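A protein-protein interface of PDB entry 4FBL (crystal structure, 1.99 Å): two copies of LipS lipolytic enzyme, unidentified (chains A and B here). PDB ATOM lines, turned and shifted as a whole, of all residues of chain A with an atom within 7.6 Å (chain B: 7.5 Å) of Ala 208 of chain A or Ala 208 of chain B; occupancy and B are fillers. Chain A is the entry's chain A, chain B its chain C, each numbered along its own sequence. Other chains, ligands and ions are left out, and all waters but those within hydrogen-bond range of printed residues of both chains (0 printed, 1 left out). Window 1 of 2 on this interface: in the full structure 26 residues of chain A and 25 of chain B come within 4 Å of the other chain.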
ATOM      1  N   ALA A 132      24.654  31.935 -21.066  1.00  0.00           N
ATOM      2  CA  ALA A 132      23.396  32.073 -20.279  1.00  0.00           C
ATOM      3  C   ALA A 132      23.658  32.648 -18.865  1.00  0.00           C
ATOM      4  O   ALA A 132      22.929  33.487 -18.358  1.00  0.00           O
ATOM      5  CB  ALA A 132      22.680  30.640 -20.176  1.00  0.00           C
ATOM      6  N   ALA A 154      23.306  29.530 -24.199  1.00  0.00           N
ATOM      7  CA  ALA A 154      22.350  28.395 -24.232  1.00  0.00           C
ATOM      8  C   ALA A 154      21.070  28.700 -23.349  1.00  0.00           C
ATOM      9  O   ALA A 154      20.879  28.121 -22.258  1.00  0.00           O
ATOM     10  CB  ALA A 154      23.031  27.161 -23.756  1.00  0.00           C
ATOM     11  N   LEU A 155      20.231  29.583 -23.852  1.00  0.00           N
ATOM     12  CA  LEU A 155      18.931  29.912 -23.206  1.00  0.00           C
ATOM     13  C   LEU A 155      17.884  28.820 -23.507  1.00  0.00           C
ATOM     14  O   LEU A 155      17.211  28.371 -22.598  1.00  0.00           O
ATOM     15  CB  LEU A 155      18.439  31.289 -23.623  1.00  0.00           C
ATOM     16  CG  LEU A 155      18.854  32.461 -22.732  1.00  0.00           C
ATOM     17  CD1 LEU A 155      20.385  32.653 -22.609  1.00  0.00           C
ATOM     18  CD2 LEU A 155      18.219  33.768 -23.247  1.00  0.00           C
ATOM     19  N   ARG A 156      17.777  28.426 -24.762  1.00  0.00           N
ATOM     20  CA  ARG A 156      16.819  27.385 -25.198  1.00  0.00           C
ATOM     21  C   ARG A 156      17.548  26.272 -25.989  1.00  0.00           C
ATOM     22  O   ARG A 156      18.008  26.494 -27.122  1.00  0.00           O
ATOM     23  CB  ARG A 156      15.745  28.018 -26.090  1.00  0.00           C
ATOM     24  CG  ARG A 156      14.782  28.969 -25.335  1.00  0.00           C
ATOM     25  CD  ARG A 156      13.831  29.711 -26.327  1.00  0.00           C
ATOM     26  NE  ARG A 156      12.797  28.808 -26.781  1.00  0.00           N
ATOM     27  CZ  ARG A 156      11.778  28.386 -26.012  1.00  0.00           C
ATOM     28  NH1 ARG A 156      11.620  28.839 -24.750  1.00  0.00           N
ATOM     29  NH2 ARG A 156      10.898  27.530 -26.516  1.00  0.00           N
ATOM     30  N   ALA A 163      15.302  17.179 -22.858  1.00  0.00           N
ATOM     31  CA  ALA A 163      14.258  17.402 -21.789  1.00  0.00           C
ATOM     32  C   ALA A 163      13.813  16.025 -21.206  1.00  0.00           C
ATOM     33  O   ALA A 163      13.608  15.904 -19.985  1.00  0.00           O
ATOM     34  CB  ALA A 163      13.059  18.161 -22.332  1.00  0.00           C
ATOM     35  N   LYS A 201      19.192  18.787 -15.806  1.00  0.00           N
ATOM     36  CA  LYS A 201      18.104  19.673 -15.395  1.00  0.00           C
ATOM     37  C   LYS A 201      18.639  21.103 -15.077  1.00  0.00           C
ATOM     38  O   LYS A 201      17.918  22.073 -15.289  1.00  0.00           O
ATOM     39  CB  LYS A 201      17.358  19.093 -14.152  1.00  0.00           C
ATOM     40  CG  LYS A 201      18.252  18.818 -12.933  1.00  0.00           C
ATOM     41  CD  LYS A 201      17.451  17.935 -11.949  1.00  0.00           C
ATOM     42  CE  LYS A 201      18.267  17.142 -10.963  1.00  0.00           C
ATOM     43  NZ  LYS A 201      18.766  15.836 -11.559  1.00  0.00           N
ATOM     44  N   HIS A 202      19.846  21.181 -14.523  1.00  0.00           N
ATOM     45  CA  HIS A 202      20.455  22.421 -14.128  1.00  0.00           C
ATOM     46  C   HIS A 202      20.887  23.346 -15.320  1.00  0.00           C
ATOM     47  O   HIS A 202      20.824  24.585 -15.210  1.00  0.00           O
ATOM     48  CB  HIS A 202      21.615  22.001 -13.259  1.00  0.00           C
ATOM     49  CG  HIS A 202      21.154  21.453 -11.942  1.00  0.00           C
ATOM     50  ND1 HIS A 202      21.383  20.140 -11.527  1.00  0.00           N
ATOM     51  CD2 HIS A 202      20.419  22.032 -10.971  1.00  0.00           C
ATOM     52  CE1 HIS A 202      20.841  19.953 -10.337  1.00  0.00           C
ATOM     53  NE2 HIS A 202      20.317  21.107  -9.938  1.00  0.00           N
ATOM     54  N   LEU A 203      21.323  22.736 -16.431  1.00  0.00           N
ATOM     55  CA  LEU A 203      21.496  23.459 -17.681  1.00  0.00           C
ATOM     56  C   LEU A 203      20.216  24.098 -18.155  1.00  0.00           C
ATOM     57  O   LEU A 203      20.207  25.236 -18.724  1.00  0.00           O
ATOM     58  CB  LEU A 203      21.988  22.497 -18.802  1.00  0.00           C
ATOM     59  CG  LEU A 203      22.133  22.949 -20.238  1.00  0.00           C
ATOM     60  CD1 LEU A 203      23.175  24.111 -20.377  1.00  0.00           C
ATOM     61  CD2 LEU A 203      22.479  21.734 -21.202  1.00  0.00           C
ATOM     62  N   ILE A 204      19.166  23.290 -18.154  1.00  0.00           N
ATOM     63  CA  ILE A 204      17.893  23.757 -18.667  1.00  0.00           C
ATOM     64  C   ILE A 204      17.372  24.870 -17.675  1.00  0.00           C
ATOM     65  O   ILE A 204      16.883  25.898 -18.118  1.00  0.00           O
ATOM     66  CB  ILE A 204      16.896  22.613 -18.754  1.00  0.00           C
ATOM     67  CG1 ILE A 204      17.320  21.619 -19.840  1.00  0.00           C
ATOM     68  CG2 ILE A 204      15.394  23.154 -18.902  1.00  0.00           C
ATOM     69  CD1 ILE A 204      16.397  20.352 -19.904  1.00  0.00           C
ATOM     70  N   THR A 205      17.555  24.691 -16.375  1.00  0.00           N
ATOM     71  CA  THR A 205      17.114  25.735 -15.466  1.00  0.00           C
ATOM     72  C   THR A 205      17.834  27.100 -15.640  1.00  0.00           C
ATOM     73  O   THR A 205      17.205  28.194 -15.576  1.00  0.00           O
ATOM     74  CB  THR A 205      17.409  25.289 -13.976  1.00  0.00           C
ATOM     75  OG1 THR A 205      16.687  24.094 -13.701  1.00  0.00           O
ATOM     76  CG2 THR A 205      16.946  26.325 -12.962  1.00  0.00           C
ATOM     77  N   ILE A 206      19.154  27.048 -15.789  1.00  0.00           N
ATOM     78  CA  ILE A 206      19.905  28.323 -15.962  1.00  0.00           C
ATOM     79  C   ILE A 206      19.423  28.976 -17.216  1.00  0.00           C
ATOM     80  O   ILE A 206      19.230  30.148 -17.224  1.00  0.00           O
ATOM     81  CB  ILE A 206      21.425  28.130 -16.129  1.00  0.00           C
ATOM     82  CG1 ILE A 206      22.072  27.537 -14.876  1.00  0.00           C
ATOM     83  CG2 ILE A 206      22.112  29.447 -16.610  1.00  0.00           C
ATOM     84  CD1 ILE A 206      22.080  28.463 -13.789  1.00  0.00           C
ATOM     85  N   GLY A 207      19.262  28.217 -18.320  1.00  0.00           N
ATOM     86  CA  GLY A 207      18.785  28.855 -19.523  1.00  0.00           C
ATOM     87  C   GLY A 207      17.397  29.567 -19.373  1.00  0.00           C
ATOM     88  O   GLY A 207      17.142  30.692 -19.915  1.00  0.00           O
ATOM     89  N   ALA A 208      16.505  28.865 -18.666  1.00  0.00           N
ATOM     90  CA  ALA A 208      15.105  29.351 -18.461  1.00  0.00           C
ATOM     91  C   ALA A 208      15.097  30.587 -17.609  1.00  0.00           C
ATOM     92  O   ALA A 208      14.385  31.516 -17.894  1.00  0.00           O
ATOM     93  CB  ALA A 208      14.242  28.230 -17.770  1.00  0.00           C
ATOM     94  N   VAL A 209      15.870  30.608 -16.543  1.00  0.00           N
ATOM     95  CA  VAL A 209      15.912  31.788 -15.719  1.00  0.00           C
ATOM     96  C   VAL A 209      16.521  33.010 -16.489  1.00  0.00           C
ATOM     97  O   VAL A 209      15.895  34.082 -16.575  1.00  0.00           O
ATOM     98  CB  VAL A 209      16.631  31.463 -14.438  1.00  0.00           C
ATOM     99  CG1 VAL A 209      16.883  32.748 -13.578  1.00  0.00           C
ATOM    100  CG2 VAL A 209      15.785  30.516 -13.670  1.00  0.00           C
ATOM    101  N   ALA A 210      17.626  32.776 -17.235  1.00  0.00           N
ATOM    102  CA  ALA A 210      18.186  33.820 -18.016  1.00  0.00           C
ATOM    103  C   ALA A 210      17.187  34.288 -19.061  1.00  0.00           C
ATOM    104  O   ALA A 210      17.056  35.512 -19.269  1.00  0.00           O
ATOM    105  CB  ALA A 210      19.565  33.338 -18.719  1.00  0.00           C
ATOM    106  N   GLU A 211      16.461  33.395 -19.746  1.00  0.00           N
ATOM    107  CA  GLU A 211      15.562  33.958 -20.760  1.00  0.00           C
ATOM    108  C   GLU A 211      14.468  34.913 -20.128  1.00  0.00           C
ATOM    109  O   GLU A 211      14.103  35.921 -20.667  1.00  0.00           O
ATOM    110  CB  GLU A 211      14.904  32.822 -21.561  1.00  0.00           C
ATOM    111  CG  GLU A 211      13.729  33.334 -22.448  1.00  0.00           C
ATOM    112  CD  GLU A 211      13.024  32.310 -23.336  1.00  0.00           C
ATOM    113  OE1 GLU A 211      13.318  31.106 -23.294  1.00  0.00           O
ATOM    114  OE2 GLU A 211      12.120  32.720 -24.117  1.00  0.00           O
ATOM    115  N   MET A 212      13.962  34.552 -18.959  1.00  0.00           N
ATOM    116  CA  MET A 212      12.848  35.276 -18.283  1.00  0.00           C
ATOM    117  C   MET A 212      13.398  36.596 -17.732  1.00  0.00           C
ATOM    118  O   MET A 212      12.617  37.561 -17.448  1.00  0.00           O
ATOM    119  CB  MET A 212      12.324  34.446 -17.103  1.00  0.00           C
ATOM    120  CG  MET A 212      10.865  34.888 -16.575  1.00  0.00           C
ATOM    121  SD  MET A 212      10.211  33.848 -15.255  1.00  0.00           S
ATOM    122  CE  MET A 212      10.205  32.179 -16.008  1.00  0.00           C
ATOM    123  N   LEU A 213      14.729  36.656 -17.565  1.00  0.00           N
ATOM    124  CA  LEU A 213      15.360  37.870 -17.026  1.00  0.00           C
ATOM    125  C   LEU A 213      15.703  38.870 -18.119  1.00  0.00           C
ATOM    126  O   LEU A 213      16.039  40.079 -17.843  1.00  0.00           O
ATOM    127  CB  LEU A 213      16.620  37.530 -16.212  1.00  0.00           C
ATOM    128  CG  LEU A 213      16.546  37.091 -14.784  1.00  0.00           C
ATOM    129  CD1 LEU A 213      17.943  36.657 -14.225  1.00  0.00           C
ATOM    130  CD2 LEU A 213      15.916  38.244 -13.965  1.00  0.00           C
ATOM    131  N   LEU A 214      15.603  38.455 -19.376  1.00  0.00           N
ATOM    132  CA  LEU A 214      16.022  39.318 -20.491  1.00  0.00           C
ATOM    133  C   LEU A 214      15.563  40.803 -20.428  1.00  0.00           C
ATOM    134  O   LEU A 214      16.347  41.683 -20.794  1.00  0.00           O
ATOM    135  CB  LEU A 214      15.614  38.704 -21.817  1.00  0.00           C
ATOM    136  CG  LEU A 214      16.481  37.582 -22.483  1.00  0.00           C
ATOM    137  CD1 LEU A 214      15.747  36.988 -23.689  1.00  0.00           C
ATOM    138  CD2 LEU A 214      17.971  38.074 -22.870  1.00  0.00           C
ATOM    139  N   ALA B 132       1.570  21.770 -15.478  1.00  0.00           N
ATOM    140  CA  ALA B 132       2.896  21.631 -16.161  1.00  0.00           C
ATOM    141  C   ALA B 132       3.455  20.217 -15.908  1.00  0.00           C
ATOM    142  O   ALA B 132       4.058  19.598 -16.814  1.00  0.00           O
ATOM    143  CB  ALA B 132       3.908  22.716 -15.572  1.00  0.00           C
ATOM    144  N   ALA B 154       1.358  26.035 -15.865  1.00  0.00           N
ATOM    145  CA  ALA B 154       2.383  27.069 -15.639  1.00  0.00           C
ATOM    146  C   ALA B 154       3.725  26.686 -16.357  1.00  0.00           C
ATOM    147  O   ALA B 154       4.737  26.320 -15.727  1.00  0.00           O
ATOM    148  CB  ALA B 154       2.601  27.239 -14.136  1.00  0.00           C
ATOM    149  N   LEU B 155       3.686  26.673 -17.663  1.00  0.00           N
ATOM    150  CA  LEU B 155       4.951  26.375 -18.473  1.00  0.00           C
ATOM    151  C   LEU B 155       5.880  27.616 -18.528  1.00  0.00           C
ATOM    152  O   LEU B 155       7.113  27.481 -18.357  1.00  0.00           O
ATOM    153  CB  LEU B 155       4.595  25.912 -19.844  1.00  0.00           C
ATOM    154  CG  LEU B 155       4.416  24.386 -20.036  1.00  0.00           C
ATOM    155  CD1 LEU B 155       3.278  23.793 -19.257  1.00  0.00           C
ATOM    156  CD2 LEU B 155       4.068  24.186 -21.491  1.00  0.00           C
ATOM    157  N   ARG B 156       5.276  28.801 -18.733  1.00  0.00           N
ATOM    158  CA  ARG B 156       6.011  30.107 -18.868  1.00  0.00           C
ATOM    159  C   ARG B 156       5.369  31.139 -17.962  1.00  0.00           C
ATOM    160  O   ARG B 156       4.237  31.557 -18.233  1.00  0.00           O
ATOM    161  CB  ARG B 156       5.945  30.564 -20.317  1.00  0.00           C
ATOM    162  CG  ARG B 156       6.643  29.632 -21.288  1.00  0.00           C
ATOM    163  CD  ARG B 156       6.620  30.291 -22.780  1.00  0.00           C
ATOM    164  NE  ARG B 156       7.952  30.754 -23.173  1.00  0.00           N
ATOM    165  CZ  ARG B 156       8.452  31.975 -22.967  1.00  0.00           C
ATOM    166  NH1 ARG B 156       7.724  32.951 -22.410  1.00  0.00           N
ATOM    167  NH2 ARG B 156       9.684  32.249 -23.346  1.00  0.00           N
ATOM    168  N   ALA B 163      11.843  35.588 -11.806  1.00  0.00           N
ATOM    169  CA  ALA B 163      13.138  35.029 -12.291  1.00  0.00           C
ATOM    170  C   ALA B 163      14.288  35.652 -11.449  1.00  0.00           C
ATOM    171  O   ALA B 163      15.269  34.974 -11.118  1.00  0.00           O
ATOM    172  CB  ALA B 163      13.251  35.310 -13.782  1.00  0.00           C
ATOM    173  N   LYS B 201      13.003  28.495  -7.934  1.00  0.00           N
ATOM    174  CA  LYS B 201      13.830  27.978  -9.050  1.00  0.00           C
ATOM    175  C   LYS B 201      13.202  26.640  -9.645  1.00  0.00           C
ATOM    176  O   LYS B 201      13.113  26.455 -10.877  1.00  0.00           O
ATOM    177  CB  LYS B 201      15.285  27.808  -8.589  1.00  0.00           C
ATOM    178  CG  LYS B 201      15.543  26.671  -7.663  1.00  0.00           C
ATOM    179  CD  LYS B 201      17.003  26.534  -7.166  1.00  0.00           C
ATOM    180  CE  LYS B 201      17.419  27.700  -6.247  1.00  0.00           C
ATOM    181  NZ  LYS B 201      16.858  27.608  -4.836  1.00  0.00           N
ATOM    182  N   HIS B 202      12.662  25.814  -8.748  1.00  0.00           N
ATOM    183  CA  HIS B 202      11.963  24.562  -9.119  1.00  0.00           C
ATOM    184  C   HIS B 202      10.683  24.748  -9.857  1.00  0.00           C
ATOM    185  O   HIS B 202      10.372  23.926 -10.745  1.00  0.00           O
ATOM    186  CB  HIS B 202      11.792  23.796  -7.814  1.00  0.00           C
ATOM    187  CG  HIS B 202      13.127  23.493  -7.233  1.00  0.00           C
ATOM    188  ND1 HIS B 202      13.578  23.971  -6.006  1.00  0.00           N
ATOM    189  CD2 HIS B 202      14.135  22.749  -7.745  1.00  0.00           C
ATOM    190  CE1 HIS B 202      14.815  23.545  -5.797  1.00  0.00           C
ATOM    191  NE2 HIS B 202      15.168  22.776  -6.834  1.00  0.00           N
ATOM    192  N   LEU B 203       9.898  25.787  -9.538  1.00  0.00           N
ATOM    193  CA  LEU B 203       8.755  26.070 -10.361  1.00  0.00           C
ATOM    194  C   LEU B 203       9.146  26.337 -11.785  1.00  0.00           C
ATOM    195  O   LEU B 203       8.491  25.864 -12.763  1.00  0.00           O
ATOM    196  CB  LEU B 203       7.959  27.261  -9.812  1.00  0.00           C
ATOM    197  CG  LEU B 203       6.830  27.909 -10.639  1.00  0.00           C
ATOM    198  CD1 LEU B 203       5.650  27.039 -10.951  1.00  0.00           C
ATOM    199  CD2 LEU B 203       6.252  29.247 -10.002  1.00  0.00           C
ATOM    200  N   ILE B 204      10.169  27.167 -11.979  1.00  0.00           N
ATOM    201  CA  ILE B 204      10.551  27.594 -13.353  1.00  0.00           C
ATOM    202  C   ILE B 204      11.145  26.350 -14.117  1.00  0.00           C
ATOM    203  O   ILE B 204      10.871  26.176 -15.307  1.00  0.00           O
ATOM    204  CB  ILE B 204      11.645  28.757 -13.273  1.00  0.00           C
ATOM    205  CG1 ILE B 204      10.956  30.109 -12.942  1.00  0.00           C
ATOM    206  CG2 ILE B 204      12.306  28.929 -14.620  1.00  0.00           C
ATOM    207  CD1 ILE B 204      11.866  31.199 -12.312  1.00  0.00           C
ATOM    208  N   THR B 205      11.882  25.512 -13.404  1.00  0.00           N
ATOM    209  CA  THR B 205      12.537  24.330 -13.996  1.00  0.00           C
ATOM    210  C   THR B 205      11.446  23.394 -14.595  1.00  0.00           C
ATOM    211  O   THR B 205      11.472  22.998 -15.805  1.00  0.00           O
ATOM    212  CB  THR B 205      13.389  23.499 -12.949  1.00  0.00           C
ATOM    213  OG1 THR B 205      14.514  24.280 -12.465  1.00  0.00           O
ATOM    214  CG2 THR B 205      13.942  22.207 -13.625  1.00  0.00           C
ATOM    215  N   ILE B 206      10.420  23.086 -13.758  1.00  0.00           N
ATOM    216  CA  ILE B 206       9.340  22.216 -14.221  1.00  0.00           C
ATOM    217  C   ILE B 206       8.685  22.815 -15.426  1.00  0.00           C
ATOM    218  O   ILE B 206       8.388  22.081 -16.387  1.00  0.00           O
ATOM    219  CB  ILE B 206       8.200  21.974 -13.141  1.00  0.00           C
ATOM    220  CG1 ILE B 206       8.718  21.280 -11.907  1.00  0.00           C
ATOM    221  CG2 ILE B 206       7.039  21.122 -13.796  1.00  0.00           C
ATOM    222  CD1 ILE B 206       9.141  19.958 -12.258  1.00  0.00           C
ATOM    223  N   GLY B 207       8.377  24.130 -15.378  1.00  0.00           N
ATOM    224  CA  GLY B 207       7.733  24.700 -16.519  1.00  0.00           C
ATOM    225  C   GLY B 207       8.585  24.590 -17.797  1.00  0.00           C
ATOM    226  O   GLY B 207       8.091  24.288 -18.929  1.00  0.00           O
ATOM    227  N   ALA B 208       9.869  24.870 -17.659  1.00  0.00           N
ATOM    228  CA  ALA B 208      10.759  24.758 -18.859  1.00  0.00           C
ATOM    229  C   ALA B 208      10.941  23.303 -19.431  1.00  0.00           C
ATOM    230  O   ALA B 208      10.982  23.096 -20.654  1.00  0.00           O
ATOM    231  CB  ALA B 208      12.110  25.355 -18.542  1.00  0.00           C
ATOM    232  N   VAL B 209      11.076  22.322 -18.539  1.00  0.00           N
ATOM    233  CA  VAL B 209      11.230  20.940 -18.976  1.00  0.00           C
ATOM    234  C   VAL B 209       9.951  20.541 -19.717  1.00  0.00           C
ATOM    235  O   VAL B 209      10.007  19.992 -20.828  1.00  0.00           O
ATOM    236  CB  VAL B 209      11.596  19.984 -17.835  1.00  0.00           C
ATOM    237  CG1 VAL B 209      11.462  18.471 -18.314  1.00  0.00           C
ATOM    238  CG2 VAL B 209      13.052  20.307 -17.334  1.00  0.00           C
ATOM    239  N   ALA B 210       8.782  20.909 -19.166  1.00  0.00           N
ATOM    240  CA  ALA B 210       7.495  20.590 -19.837  1.00  0.00           C
ATOM    241  C   ALA B 210       7.368  21.204 -21.156  1.00  0.00           C
ATOM    242  O   ALA B 210       6.891  20.515 -22.138  1.00  0.00           O
ATOM    243  CB  ALA B 210       6.238  21.032 -18.951  1.00  0.00           C
ATOM    244  N   GLU B 211       7.651  22.525 -21.212  1.00  0.00           N
ATOM    245  CA  GLU B 211       7.648  23.173 -22.498  1.00  0.00           C
ATOM    246  C   GLU B 211       8.536  22.440 -23.549  1.00  0.00           C
ATOM    247  O   GLU B 211       8.149  22.310 -24.722  1.00  0.00           O
ATOM    248  CB  GLU B 211       8.114  24.633 -22.393  1.00  0.00           C
ATOM    249  CG  GLU B 211       7.810  25.332 -23.763  1.00  0.00           C
ATOM    250  CD  GLU B 211       8.216  26.877 -23.790  1.00  0.00           C
ATOM    251  OE1 GLU B 211       8.522  27.445 -22.758  1.00  0.00           O
ATOM    252  OE2 GLU B 211       8.187  27.520 -24.846  1.00  0.00           O
ATOM    253  N   MET B 212       9.753  22.074 -23.169  1.00  0.00           N
ATOM    254  CA  MET B 212      10.680  21.418 -24.123  1.00  0.00           C
ATOM    255  C   MET B 212      10.207  19.973 -24.567  1.00  0.00           C
ATOM    256  O   MET B 212      10.483  19.522 -25.698  1.00  0.00           O
ATOM    257  CB  MET B 212      12.070  21.333 -23.473  1.00  0.00           C
ATOM    258  CG  MET B 212      13.219  21.155 -24.556  1.00  0.00           C
ATOM    259  SD  MET B 212      14.880  21.129 -23.892  1.00  0.00           S
ATOM    260  CE  MET B 212      14.858  22.669 -22.859  1.00  0.00           C
ATOM    261  N   LEU B 213       9.463  19.274 -23.680  1.00  0.00           N
ATOM    262  CA  LEU B 213       8.803  18.005 -24.033  1.00  0.00           C
ATOM    263  C   LEU B 213       7.542  18.044 -24.936  1.00  0.00           C
ATOM    264  O   LEU B 213       7.122  16.998 -25.460  1.00  0.00           O
ATOM    265  CB  LEU B 213       8.404  17.308 -22.760  1.00  0.00           C
ATOM    266  CG  LEU B 213       9.538  16.783 -21.935  1.00  0.00           C
ATOM    267  CD1 LEU B 213       9.055  16.216 -20.532  1.00  0.00           C
ATOM    268  CD2 LEU B 213      10.225  15.628 -22.677  1.00  0.00           C
ATOM    269  N   LEU B 214       6.931  19.210 -25.123  1.00  0.00           N
ATOM    270  CA  LEU B 214       5.699  19.297 -25.822  1.00  0.00           C
ATOM    271  C   LEU B 214       5.581  18.430 -27.114  1.00  0.00           C
ATOM    272  O   LEU B 214       4.581  17.772 -27.284  1.00  0.00           O
ATOM    273  CB  LEU B 214       5.379  20.758 -26.120  1.00  0.00           C
ATOM    274  CG  LEU B 214       4.751  21.616 -24.990  1.00  0.00           C
ATOM    275  CD1 LEU B 214       4.757  23.157 -25.304  1.00  0.00           C
ATOM    276  CD2 LEU B 214       3.340  21.185 -24.663  1.00  0.00           C
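Of chain B, only Ile 204 (3.8 Å) and Ala 208 (3.7 Å) come within 4 Å of Ala 208 of chain A.
Of chain A, only Ile 204 and Ala 208 come within 4 Å of Ala 208 of chain B.
No residue of chain B comes within 4 Å of Gly 207 of chain A.
No residue of chain A comes within 4 Å of Gly 207 of chain B.
Of the printed residues of chain A, Val 209 of chain B touches Ala 163.
Of the printed residues of chain A, Ile 204 of chain B touches Ala 208 (3.8 Å), Val 209 (3.9 Å) and Met 212 (3.8 Å).
Leu 155 of chain A touches none of the printed residues of chain B.
Leu 203 of chain B touches none of the printed residues of chain A.
The nearest residue of chain B that does not touch Ala 208 of chain A is Thr 205 of chain B (5.7 Å).
The nearest residue of chain A that does not touch Ala 208 of chain B is Ala 163 of chain A (5.6 Å).
The nearest printed residue of chain B that does not touch Met 212 of chain A is Arg 156 of chain B (5.3 Å).
Hydrophobic or aromatic side chains of chain A within 4 Å of the printed part of chain B: Ala 163, Ile 204, Ala 208, Val 209, Met 212 and Leu 213.
Printed residues of chain B that touch a printed residue of chain A: Arg 156, Ala 163, Ile 204, Thr 205, Ala 208, Val 209, Glu 211, Met 212 and Leu 213.
Among the printed residues, 14 pairs touch across the chains.
Ile 204 of chain A touches Ala 208 of chain B, and with the chains exchanged Ala 208 of chain A touches Ile 204 of chain B.
Thr 205 of chain A touches its own counterpart, Thr 205 of chain B.
Ala 208 of chain B touches its own counterpart, Ala 208 of chain A.
Met 212 of chain A touches Ile 204 of chain B, but with the chains exchanged Ile 204 of chain A does not touch Met 212 of chain B (4.02 Å).
Of the 14 pairs that touch across the chains among the printed residues, 12 have their exchanged pair printed and touching as well.
Among the printed residues, merely in contact across the chains: Ala 163 of chain A with Met 212 of chain B, Met 212 of chain A with Ala 163 of chain B, Ala 208 of chain A with Ala 208 of chain B, Val 209 of chain A with Ala 163 of chain B, Ala 163 of chain A with Val 209 of chain B, Ala 208 of chain A with Ile 204 of chain B, Met 212 of chain A with Ile 204 of chain B, Ala 163 of chain A with Leu 213 of chain B, Leu 213 of chain A with Ala 163 of chain B, Val 209 of chain A with Ile 204 of chain B and Ile 204 of chain A with Ala 208 of chain B.
OE1 of Glu 211 of chain A is in salt-bridge range of NH1 of Arg 156 of chain A (3.2 Å).
The side-chain hydroxyl of Thr 205 of chain A is in hydrogen-bond range of the backbone carbonyl oxygen of Lys 201 of chain A (2.8 Å).
The side-chain hydroxyl (OG1) of Thr 205 of chain B is in hydrogen-bond range of the backbone carbonyl oxygen (O) of Lys 201 of chain B, 3.0 Å away.
The side-chain carboxylate (OE1) of Glu 211 of chain B is in salt-bridge range of the guanidinium group (NE) of Arg 156 of chain B, at 3.4 Å.
OG1 of Thr 205 of chain A is in hydrogen-bond range of OG1 of Thr 205 of chain B, 2.5 Å away.
NH2 of Arg 156 of chain A is in salt-bridge range of OE2 of Glu 211 of chain B.
OE2 of Glu 211 of chain A is in salt-bridge range of NH2 of Arg 156 of chain B (2.6 Å).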
